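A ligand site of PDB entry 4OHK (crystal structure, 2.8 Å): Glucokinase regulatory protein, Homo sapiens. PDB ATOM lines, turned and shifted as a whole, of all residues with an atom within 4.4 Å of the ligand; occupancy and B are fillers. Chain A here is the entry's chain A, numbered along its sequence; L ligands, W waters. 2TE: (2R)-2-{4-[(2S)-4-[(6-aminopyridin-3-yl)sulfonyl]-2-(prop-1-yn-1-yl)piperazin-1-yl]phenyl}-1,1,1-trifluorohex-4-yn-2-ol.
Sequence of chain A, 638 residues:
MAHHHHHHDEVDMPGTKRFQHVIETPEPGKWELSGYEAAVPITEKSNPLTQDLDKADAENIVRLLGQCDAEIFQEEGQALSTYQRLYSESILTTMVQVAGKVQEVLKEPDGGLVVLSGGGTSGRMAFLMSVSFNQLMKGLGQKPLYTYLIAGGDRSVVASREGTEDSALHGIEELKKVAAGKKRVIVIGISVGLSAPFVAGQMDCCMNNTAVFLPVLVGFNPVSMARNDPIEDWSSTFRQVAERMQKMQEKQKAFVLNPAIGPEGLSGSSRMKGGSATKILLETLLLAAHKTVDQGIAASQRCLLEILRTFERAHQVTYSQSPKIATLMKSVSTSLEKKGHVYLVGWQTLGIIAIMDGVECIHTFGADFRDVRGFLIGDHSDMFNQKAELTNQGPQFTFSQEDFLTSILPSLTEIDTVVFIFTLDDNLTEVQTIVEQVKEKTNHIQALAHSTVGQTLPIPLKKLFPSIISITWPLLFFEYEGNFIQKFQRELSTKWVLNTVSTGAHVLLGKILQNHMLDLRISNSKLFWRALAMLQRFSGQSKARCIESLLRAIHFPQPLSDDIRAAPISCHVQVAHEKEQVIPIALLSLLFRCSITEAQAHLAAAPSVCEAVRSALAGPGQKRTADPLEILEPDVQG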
ATOM      1  N   VAL A  22     -28.123 -31.982  11.391  1.00  0.00           N
ATOM      2  CA  VAL A  22     -27.743 -31.251  12.588  1.00  0.00           C
ATOM      3  C   VAL A  22     -27.200 -32.206  13.636  1.00  0.00           C
ATOM      4  O   VAL A  22     -27.873 -33.152  13.986  1.00  0.00           O
ATOM      5  CB  VAL A  22     -28.941 -30.487  13.188  1.00  0.00           C
ATOM      6  CG1 VAL A  22     -28.572 -29.839  14.514  1.00  0.00           C
ATOM      7  CG2 VAL A  22     -29.429 -29.446  12.206  1.00  0.00           C
ATOM      8  N   TYR A  36     -18.268 -33.616  18.666  1.00  0.00           N
ATOM      9  CA  TYR A  36     -19.122 -32.511  18.210  1.00  0.00           C
ATOM     10  C   TYR A  36     -18.240 -31.359  17.783  1.00  0.00           C
ATOM     11  O   TYR A  36     -18.402 -30.821  16.680  1.00  0.00           O
ATOM     12  CB  TYR A  36     -20.070 -32.017  19.302  1.00  0.00           C
ATOM     13  CG  TYR A  36     -20.991 -30.889  18.885  1.00  0.00           C
ATOM     14  CD1 TYR A  36     -20.553 -29.564  18.869  1.00  0.00           C
ATOM     15  CD2 TYR A  36     -22.291 -31.122  18.494  1.00  0.00           C
ATOM     16  CE1 TYR A  36     -21.390 -28.535  18.484  1.00  0.00           C
ATOM     17  CE2 TYR A  36     -23.137 -30.089  18.109  1.00  0.00           C
ATOM     18  CZ  TYR A  36     -22.668 -28.790  18.111  1.00  0.00           C
ATOM     19  OH  TYR A  36     -23.495 -27.762  17.716  1.00  0.00           O
ATOM     20  N   VAL A  40     -17.600 -28.421  14.235  1.00  0.00           N
ATOM     21  CA  VAL A  40     -17.914 -27.007  14.139  1.00  0.00           C
ATOM     22  C   VAL A  40     -16.858 -26.374  13.240  1.00  0.00           C
ATOM     23  O   VAL A  40     -15.699 -26.370  13.602  1.00  0.00           O
ATOM     24  CB  VAL A  40     -17.833 -26.261  15.483  1.00  0.00           C
ATOM     25  CG1 VAL A  40     -18.123 -24.781  15.300  1.00  0.00           C
ATOM     26  CG2 VAL A  40     -18.765 -26.891  16.506  1.00  0.00           C
ATOM     27  N   PRO A  41     -17.249 -25.822  12.098  1.00  0.00           N
ATOM     28  CA  PRO A  41     -16.187 -25.309  11.224  1.00  0.00           C
ATOM     29  C   PRO A  41     -15.424 -24.193  11.917  1.00  0.00           C
ATOM     30  O   PRO A  41     -15.970 -23.557  12.791  1.00  0.00           O
ATOM     31  CB  PRO A  41     -16.949 -24.779   9.989  1.00  0.00           C
ATOM     32  CG  PRO A  41     -18.399 -25.118  10.202  1.00  0.00           C
ATOM     33  CD  PRO A  41     -18.583 -25.382  11.674  1.00  0.00           C
ATOM     34  N   GLU A  44     -16.968 -20.745  12.646  1.00  0.00           N
ATOM     35  CA  GLU A  44     -18.067 -20.676  13.580  1.00  0.00           C
ATOM     36  C   GLU A  44     -17.640 -20.937  14.992  1.00  0.00           C
ATOM     37  O   GLU A  44     -18.376 -20.603  15.915  1.00  0.00           O
ATOM     38  CB  GLU A  44     -19.143 -21.674  13.169  1.00  0.00           C
ATOM     39  CG  GLU A  44     -19.615 -21.394  11.743  1.00  0.00           C
ATOM     40  CD  GLU A  44     -20.654 -20.270  11.669  1.00  0.00           C
ATOM     41  OE1 GLU A  44     -21.270 -19.941  12.688  1.00  0.00           O
ATOM     42  OE2 GLU A  44     -20.868 -19.746  10.570  1.00  0.00           O
ATOM     43  N   LYS A  45     -16.441 -21.512  15.160  1.00  0.00           N
ATOM     44  CA  LYS A  45     -15.915 -21.777  16.494  1.00  0.00           C
ATOM     45  C   LYS A  45     -15.903 -20.565  17.416  1.00  0.00           C
ATOM     46  O   LYS A  45     -16.004 -19.418  16.988  1.00  0.00           O
ATOM     47  CB  LYS A  45     -14.507 -22.408  16.450  1.00  0.00           C
ATOM     48  CG  LYS A  45     -14.483 -23.872  15.962  1.00  0.00           C
ATOM     49  CD  LYS A  45     -13.175 -24.579  16.300  1.00  0.00           C
ATOM     50  CE  LYS A  45     -12.766 -25.592  15.237  1.00  0.00           C
ATOM     51  NZ  LYS A  45     -13.462 -26.913  15.383  1.00  0.00           N
ATOM     52  N   SER A  46     -15.834 -20.864  18.709  1.00  0.00           N
ATOM     53  CA  SER A  46     -15.656 -19.893  19.764  1.00  0.00           C
ATOM     54  C   SER A  46     -14.184 -19.765  19.990  1.00  0.00           C
ATOM     55  O   SER A  46     -13.531 -20.738  20.356  1.00  0.00           O
ATOM     56  CB  SER A  46     -16.308 -20.413  21.044  1.00  0.00           C
ATOM     57  OG  SER A  46     -16.258 -19.450  22.051  1.00  0.00           O
ATOM     58  N   GLY A 193     -16.688 -19.013   4.908  1.00  0.00           N
ATOM     59  CA  GLY A 193     -17.111 -20.276   5.490  1.00  0.00           C
ATOM     60  C   GLY A 193     -17.158 -21.449   4.532  1.00  0.00           C
ATOM     61  O   GLY A 193     -17.485 -22.530   4.939  1.00  0.00           O
ATOM     62  N   LEU A 194     -16.760 -21.267   3.290  1.00  0.00           N
ATOM     63  CA  LEU A 194     -17.074 -22.218   2.255  1.00  0.00           C
ATOM     64  C   LEU A 194     -18.542 -22.592   2.413  1.00  0.00           C
ATOM     65  O   LEU A 194     -18.923 -23.785   2.415  1.00  0.00           O
ATOM     66  CB  LEU A 194     -16.148 -23.430   2.339  1.00  0.00           C
ATOM     67  CG  LEU A 194     -14.664 -23.111   2.194  1.00  0.00           C
ATOM     68  CD1 LEU A 194     -13.827 -24.386   2.204  1.00  0.00           C
ATOM     69  CD2 LEU A 194     -14.393 -22.349   0.920  1.00  0.00           C
ATOM     70  N   SER A 195     -19.345 -21.531   2.561  1.00  0.00           N
ATOM     71  CA  SER A 195     -20.755 -21.617   2.914  1.00  0.00           C
ATOM     72  C   SER A 195     -21.791 -21.067   1.903  1.00  0.00           C
ATOM     73  O   SER A 195     -22.865 -21.622   1.792  1.00  0.00           O
ATOM     74  CB  SER A 195     -20.981 -20.877   4.234  1.00  0.00           C
ATOM     75  OG  SER A 195     -22.257 -20.208   4.272  1.00  0.00           O
ATOM     76  N   ASN A 221     -11.889 -22.278   5.831  1.00  0.00           N
ATOM     77  CA  ASN A 221     -12.103 -23.550   6.461  1.00  0.00           C
ATOM     78  C   ASN A 221     -11.508 -24.634   5.571  1.00  0.00           C
ATOM     79  O   ASN A 221     -11.481 -24.516   4.330  1.00  0.00           O
ATOM     80  CB  ASN A 221     -13.590 -23.853   6.624  1.00  0.00           C
ATOM     81  CG  ASN A 221     -14.242 -23.156   7.806  1.00  0.00           C
ATOM     82  OD1 ASN A 221     -13.739 -23.187   8.938  1.00  0.00           O
ATOM     83  ND2 ASN A 221     -15.407 -22.582   7.567  1.00  0.00           N
ATOM     84  N   MET A 225     -14.643 -29.088   6.341  1.00  0.00           N
ATOM     85  CA  MET A 225     -15.616 -28.386   7.173  1.00  0.00           C
ATOM     86  C   MET A 225     -16.490 -27.480   6.279  1.00  0.00           C
ATOM     87  O   MET A 225     -17.149 -26.548   6.754  1.00  0.00           O
ATOM     88  CB  MET A 225     -14.932 -27.547   8.248  1.00  0.00           C
ATOM     89  CG  MET A 225     -14.259 -28.315   9.383  1.00  0.00           C
ATOM     90  SD  MET A 225     -13.004 -27.227  10.106  1.00  0.00           S
ATOM     91  CE  MET A 225     -12.780 -27.919  11.753  1.00  0.00           C
ATOM     92  N   ALA A 226     -16.459 -27.747   4.973  1.00  0.00           N
ATOM     93  CA  ALA A 226     -17.209 -26.929   4.034  1.00  0.00           C
ATOM     94  C   ALA A 226     -18.659 -27.202   4.266  1.00  0.00           C
ATOM     95  O   ALA A 226     -19.026 -28.343   4.444  1.00  0.00           O
ATOM     96  CB  ALA A 226     -16.852 -27.285   2.621  1.00  0.00           C
ATOM     97  N   ARG A 227     -19.485 -26.145   4.248  1.00  0.00           N
ATOM     98  CA  ARG A 227     -20.930 -26.256   4.523  1.00  0.00           C
ATOM     99  C   ARG A 227     -21.570 -27.332   3.677  1.00  0.00           C
ATOM    100  O   ARG A 227     -21.375 -27.367   2.441  1.00  0.00           O
ATOM    101  CB  ARG A 227     -21.623 -24.923   4.249  1.00  0.00           C
ATOM    102  CG  ARG A 227     -23.070 -24.861   4.662  1.00  0.00           C
ATOM    103  CD  ARG A 227     -23.646 -23.452   4.566  1.00  0.00           C
ATOM    104  NE  ARG A 227     -25.028 -23.416   5.073  1.00  0.00           N
ATOM    105  CZ  ARG A 227     -25.882 -22.415   4.919  1.00  0.00           C
ATOM    106  NH1 ARG A 227     -25.553 -21.289   4.307  1.00  0.00           N
ATOM    107  NH2 ARG A 227     -27.107 -22.531   5.418  1.00  0.00           N
ATOM    108  N   ASP A 229     -25.142 -28.632   4.230  1.00  0.00           N
ATOM    109  CA  ASP A 229     -26.602 -28.798   4.227  1.00  0.00           C
ATOM    110  C   ASP A 229     -27.133 -28.564   2.821  1.00  0.00           C
ATOM    111  O   ASP A 229     -26.473 -27.956   2.004  1.00  0.00           O
ATOM    112  CB  ASP A 229     -27.340 -27.943   5.280  1.00  0.00           C
ATOM    113  CG  ASP A 229     -26.958 -26.467   5.253  1.00  0.00           C
ATOM    114  OD1 ASP A 229     -25.782 -26.178   5.061  1.00  0.00           O
ATOM    115  OD2 ASP A 229     -27.827 -25.596   5.476  1.00  0.00           O
ATOM    116  N   HIS A 516     -20.570 -14.625  21.869  1.00  0.00           N
ATOM    117  CA  HIS A 516     -21.606 -14.902  20.878  1.00  0.00           C
ATOM    118  C   HIS A 516     -22.612 -13.757  20.890  1.00  0.00           C
ATOM    119  O   HIS A 516     -22.949 -13.215  21.954  1.00  0.00           O
ATOM    120  CB  HIS A 516     -22.336 -16.220  21.198  1.00  0.00           C
ATOM    121  CG  HIS A 516     -21.440 -17.400  21.380  1.00  0.00           C
ATOM    122  ND1 HIS A 516     -20.848 -18.058  20.314  1.00  0.00           N
ATOM    123  CD2 HIS A 516     -21.034 -18.054  22.490  1.00  0.00           C
ATOM    124  CE1 HIS A 516     -20.117 -19.054  20.779  1.00  0.00           C
ATOM    125  NE2 HIS A 516     -20.218 -19.074  22.092  1.00  0.00           N
ATOM    126  N   LYS A 526     -27.749 -19.679   6.944  1.00  0.00           N
ATOM    127  CA  LYS A 526     -26.606 -19.803   7.854  1.00  0.00           C
ATOM    128  C   LYS A 526     -26.891 -19.221   9.255  1.00  0.00           C
ATOM    129  O   LYS A 526     -26.475 -19.792  10.259  1.00  0.00           O
ATOM    130  CB  LYS A 526     -25.331 -19.200   7.222  1.00  0.00           C
ATOM    131  CG  LYS A 526     -24.220 -18.800   8.199  1.00  0.00           C
ATOM    132  CD  LYS A 526     -22.949 -18.315   7.489  1.00  0.00           C
ATOM    133  CE  LYS A 526     -23.117 -16.931   6.894  1.00  0.00           C
ATOM    134  NZ  LYS A 526     -21.896 -16.455   6.179  1.00  0.00           N
ATOM    135  N   TRP A 529     -29.135 -21.586  11.195  1.00  0.00           N
ATOM    136  CA  TRP A 529     -28.411 -22.678  11.828  1.00  0.00           C
ATOM    137  C   TRP A 529     -27.610 -22.154  12.989  1.00  0.00           C
ATOM    138  O   TRP A 529     -27.584 -22.781  14.038  1.00  0.00           O
ATOM    139  CB  TRP A 529     -27.522 -23.413  10.847  1.00  0.00           C
ATOM    140  CG  TRP A 529     -28.270 -24.007   9.735  1.00  0.00           C
ATOM    141  CD1 TRP A 529     -28.130 -23.715   8.445  1.00  0.00           C
ATOM    142  CD2 TRP A 529     -29.308 -24.988   9.818  1.00  0.00           C
ATOM    143  NE1 TRP A 529     -28.993 -24.461   7.686  1.00  0.00           N
ATOM    144  CE2 TRP A 529     -29.735 -25.249   8.512  1.00  0.00           C
ATOM    145  CE3 TRP A 529     -29.922 -25.678  10.880  1.00  0.00           C
ATOM    146  CZ2 TRP A 529     -30.726 -26.168   8.217  1.00  0.00           C
ATOM    147  CZ3 TRP A 529     -30.899 -26.614  10.581  1.00  0.00           C
ATOM    148  CH2 TRP A 529     -31.297 -26.839   9.254  1.00  0.00           C
ATOM    149  N   ARG A 530     -26.974 -20.993  12.844  1.00  0.00           N
ATOM    150  CA  ARG A 530     -26.202 -20.441  13.942  1.00  0.00           C
ATOM    151  C   ARG A 530     -27.116 -20.270  15.163  1.00  0.00           C
ATOM    152  O   ARG A 530     -26.761 -20.697  16.276  1.00  0.00           O
ATOM    153  CB  ARG A 530     -25.474 -19.129  13.551  1.00  0.00           C
ATOM    154  CG  ARG A 530     -24.556 -18.532  14.640  1.00  0.00           C
ATOM    155  CD  ARG A 530     -23.724 -17.347  14.158  1.00  0.00           C
ATOM    156  NE  ARG A 530     -22.974 -17.681  12.945  1.00  0.00           N
ATOM    157  CZ  ARG A 530     -22.674 -16.836  11.955  1.00  0.00           C
ATOM    158  NH1 ARG A 530     -23.038 -15.560  11.986  1.00  0.00           N
ATOM    159  NH2 ARG A 530     -21.998 -17.267  10.904  1.00  0.00           N
ATOM    160  N   ALA A 533     -27.660 -23.579  16.715  1.00  0.00           N
ATOM    161  CA  ALA A 533     -26.442 -24.042  17.405  1.00  0.00           C
ATOM    162  C   ALA A 533     -26.176 -23.310  18.721  1.00  0.00           C
ATOM    163  O   ALA A 533     -25.651 -23.911  19.659  1.00  0.00           O
ATOM    164  CB  ALA A 533     -25.225 -23.926  16.508  1.00  0.00           C
ATOM    165  N   MET A 534     -26.531 -22.036  18.809  1.00  0.00           N
ATOM    166  CA  MET A 534     -26.412 -21.307  20.065  1.00  0.00           C
ATOM    167  C   MET A 534     -27.370 -21.813  21.093  1.00  0.00           C
ATOM    168  O   MET A 534     -27.033 -21.859  22.266  1.00  0.00           O
ATOM    169  CB  MET A 534     -26.591 -19.829  19.874  1.00  0.00           C
ATOM    170  CG  MET A 534     -25.294 -19.178  19.441  1.00  0.00           C
ATOM    171  SD  MET A 534     -25.563 -17.441  19.213  1.00  0.00           S
ATOM    172  CE  MET A 534     -26.852 -17.494  17.980  1.00  0.00           C
ATOM    173  N   GLN A 536     -28.602 -25.015  21.310  1.00  0.00           N
ATOM    174  CA  GLN A 536     -28.072 -26.266  21.842  1.00  0.00           C
ATOM    175  C   GLN A 536     -26.940 -26.019  22.843  1.00  0.00           C
ATOM    176  O   GLN A 536     -26.942 -26.592  23.910  1.00  0.00           O
ATOM    177  CB  GLN A 536     -27.563 -27.173  20.729  1.00  0.00           C
ATOM    178  CG  GLN A 536     -28.597 -27.535  19.688  1.00  0.00           C
ATOM    179  CD  GLN A 536     -28.008 -28.352  18.570  1.00  0.00           C
ATOM    180  OE1 GLN A 536     -27.683 -27.830  17.503  1.00  0.00           O
ATOM    181  NE2 GLN A 536     -27.833 -29.619  18.835  1.00  0.00           N
ATOM    182  N   ARG A 537     -26.001 -25.146  22.514  1.00  0.00           N
ATOM    183  CA  ARG A 537     -24.876 -24.872  23.435  1.00  0.00           C
ATOM    184  C   ARG A 537     -25.305 -24.286  24.780  1.00  0.00           C
ATOM    185  O   ARG A 537     -25.011 -24.875  25.813  1.00  0.00           O
ATOM    186  CB  ARG A 537     -23.830 -23.950  22.806  1.00  0.00           C
ATOM    187  CG  ARG A 537     -22.630 -23.640  23.706  1.00  0.00           C
ATOM    188  CD  ARG A 537     -21.505 -24.643  23.632  1.00  0.00           C
ATOM    189  NE  ARG A 537     -20.928 -24.727  22.299  1.00  0.00           N
ATOM    190  CZ  ARG A 537     -19.963 -25.565  21.957  1.00  0.00           C
ATOM    191  NH1 ARG A 537     -19.431 -26.394  22.846  1.00  0.00           N
ATOM    192  NH2 ARG A 537     -19.514 -25.590  20.721  1.00  0.00           N
ATOM    193  N   PHE A 538     -25.955 -23.127  24.763  1.00  0.00           N
ATOM    194  CA  PHE A 538     -26.279 -22.447  26.009  1.00  0.00           C
ATOM    195  C   PHE A 538     -27.217 -23.265  26.884  1.00  0.00           C
ATOM    196  O   PHE A 538     -27.075 -23.232  28.091  1.00  0.00           O
ATOM    197  CB  PHE A 538     -26.888 -21.061  25.746  1.00  0.00           C
ATOM    198  CG  PHE A 538     -25.906 -20.043  25.225  1.00  0.00           C
ATOM    199  CD1 PHE A 538     -24.805 -19.667  25.972  1.00  0.00           C
ATOM    200  CD2 PHE A 538     -26.119 -19.410  24.007  1.00  0.00           C
ATOM    201  CE1 PHE A 538     -23.914 -18.715  25.510  1.00  0.00           C
ATOM    202  CE2 PHE A 538     -25.210 -18.446  23.532  1.00  0.00           C
ATOM    203  CZ  PHE A 538     -24.106 -18.107  24.274  1.00  0.00           C
HETATM  204  C23 2TE L   1     -22.690 -20.705  22.722  1.00  0.00           C
HETATM  205  C22 2TE L   1     -22.637 -21.624  21.511  1.00  0.00           C
HETATM  206  C21 2TE L   1     -22.544 -21.772  20.231  1.00  0.00           C
HETATM  207  C20 2TE L   1     -22.556 -21.906  18.783  1.00  0.00           C
HETATM  208  C12 2TE L   1     -21.567 -22.961  18.424  1.00  0.00           C
HETATM  209  C24 2TE L   1     -20.177 -22.574  18.819  1.00  0.00           C
HETATM  210  F2  2TE L   1     -19.837 -21.428  18.208  1.00  0.00           F
HETATM  211  F3  2TE L   1     -20.094 -22.413  20.139  1.00  0.00           F
HETATM  212  F1  2TE L   1     -19.487 -23.641  18.459  1.00  0.00           F
HETATM  213  O3  2TE L   1     -21.942 -24.152  19.119  1.00  0.00           O
HETATM  214  C9  2TE L   1     -21.839 -23.142  16.957  1.00  0.00           C
HETATM  215  C10 2TE L   1     -21.936 -22.016  16.135  1.00  0.00           C
HETATM  216  C11 2TE L   1     -22.253 -22.151  14.780  1.00  0.00           C
HETATM  217  C8  2TE L   1     -22.089 -24.394  16.455  1.00  0.00           C
HETATM  218  C7  2TE L   1     -22.405 -24.529  15.100  1.00  0.00           C
HETATM  219  C6  2TE L   1     -22.474 -23.436  14.246  1.00  0.00           C
HETATM  220  N1  2TE L   1     -22.852 -23.601  12.908  1.00  0.00           N
HETATM  221  C2  2TE L   1     -22.877 -24.922  12.350  1.00  0.00           C
HETATM  222  C3  2TE L   1     -22.952 -24.854  10.811  1.00  0.00           C
HETATM  223  C13 2TE L   1     -24.129 -25.483  12.871  1.00  0.00           C
HETATM  224  C14 2TE L   1     -25.238 -25.791  13.252  1.00  0.00           C
HETATM  225  C15 2TE L   1     -26.565 -26.105  13.744  1.00  0.00           C
HETATM  226  C1  2TE L   1     -23.624 -22.517  12.225  1.00  0.00           C
HETATM  227  C4  2TE L   1     -23.611 -22.626  10.693  1.00  0.00           C
HETATM  228  N2  2TE L   1     -24.022 -23.971  10.356  1.00  0.00           N
HETATM  229  S1  2TE L   1     -24.044 -23.996   8.798  1.00  0.00           S
HETATM  230  O1  2TE L   1     -24.761 -25.214   8.364  1.00  0.00           O
HETATM  231  O2  2TE L   1     -24.756 -22.769   8.356  1.00  0.00           O
HETATM  232  C5  2TE L   1     -22.403 -23.991   8.149  1.00  0.00           C
HETATM  233  C19 2TE L   1     -21.800 -22.790   7.775  1.00  0.00           C
HETATM  234  C18 2TE L   1     -20.491 -22.814   7.289  1.00  0.00           C
HETATM  235  C17 2TE L   1     -19.828 -24.037   7.212  1.00  0.00           C
HETATM  236  N4  2TE L   1     -18.600 -24.065   6.760  1.00  0.00           N
HETATM  237  N3  2TE L   1     -20.442 -25.195   7.545  1.00  0.00           N
HETATM  238  C16 2TE L   1     -21.685 -25.194   8.014  1.00  0.00           C
HETATM  239  O   HOH W   1     -19.808 -27.999   8.565  1.00  0.00           O
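O of Leu 194 sits at hydrogen-bond distance from N of Arg 227 (3.0 Å). The backbone carbonyl oxygen (O) of Gly 193 lies within hydrogen-bond range of the side-chain amide nitrogen (ND2) of Asn 221, 3.4 Å away. OE2 of Glu 44 is in salt-bridge range of NH2 of Arg 530, at 2.7 Å. NE of Arg 227 lies within salt-bridge range of OD1 of Asp 229. The side-chain carboxylate (OD2) of Asp 229 sits at hydrogen-bond distance from the indole nitrogen (NE1) of Trp 529 (2.7 Å). The backbone carbonyl oxygen of Val 40 sits at hydrogen-bond distance from the side-chain amino group of Lys 45 (2.9 Å). The guanidinium group (NH1) of Arg 227 lies within hydrogen-bond range of the side-chain hydroxyl (OG) of Ser 195.
A fluorine (F2) of the ligand lies close to the backbone carbonyl oxygen (O) of Glu 44 (2.8 Å). Tyr 36 touches the ligand. CG1 of Val 40 touches F1 of the ligand (3.6 Å). Pro 41 touches the ligand (CG to N3, 3.4 Å). Ser 195 touches the ligand. Asn 221 touches the ligand. OD1 of Asp 229 touches O1 of the ligand (3.6 Å). His 516 touches the ligand. Lys 526 touches the ligand (CA to O2, 3.5 Å). O of Trp 529 touches C15 of the ligand (3.5 Å). Arg 530 touches the ligand (CA to C1, 3.7 Å). Ala 533 touches the ligand. Met 534 touches the ligand. Phe 538 touches the ligand (CZ to C23, 3.3 Å). Hydrophobic or aromatic side chains within 4 Å of the ligand: Val 40, Pro 41, His 516, Trp 529, Ala 533, Met 534 and Phe 538. Of the 24 residues printed, 18 come within 4 Å of the ligand. Along chain A the residues within 4 Å of the ligand span positions 36 to 538. The nearest printed residue that does not touch the ligand is Ala 226 (4.01 Å).
An oxygen (O3) of the ligand is in hydrogen-bond range of the guanidinium group (NH2) of Arg 537. O of Gly 193 sits at hydrogen-bond distance from N4 of the ligand (2.6 Å). The guanidinium group of Arg 227 sits at hydrogen-bond distance from an oxygen (O2) of the ligand (3.4 Å). The backbone carbonyl oxygen (O) of Met 225 sits at hydrogen-bond distance from a nitrogen (N4) of the ligand (2.9 Å).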
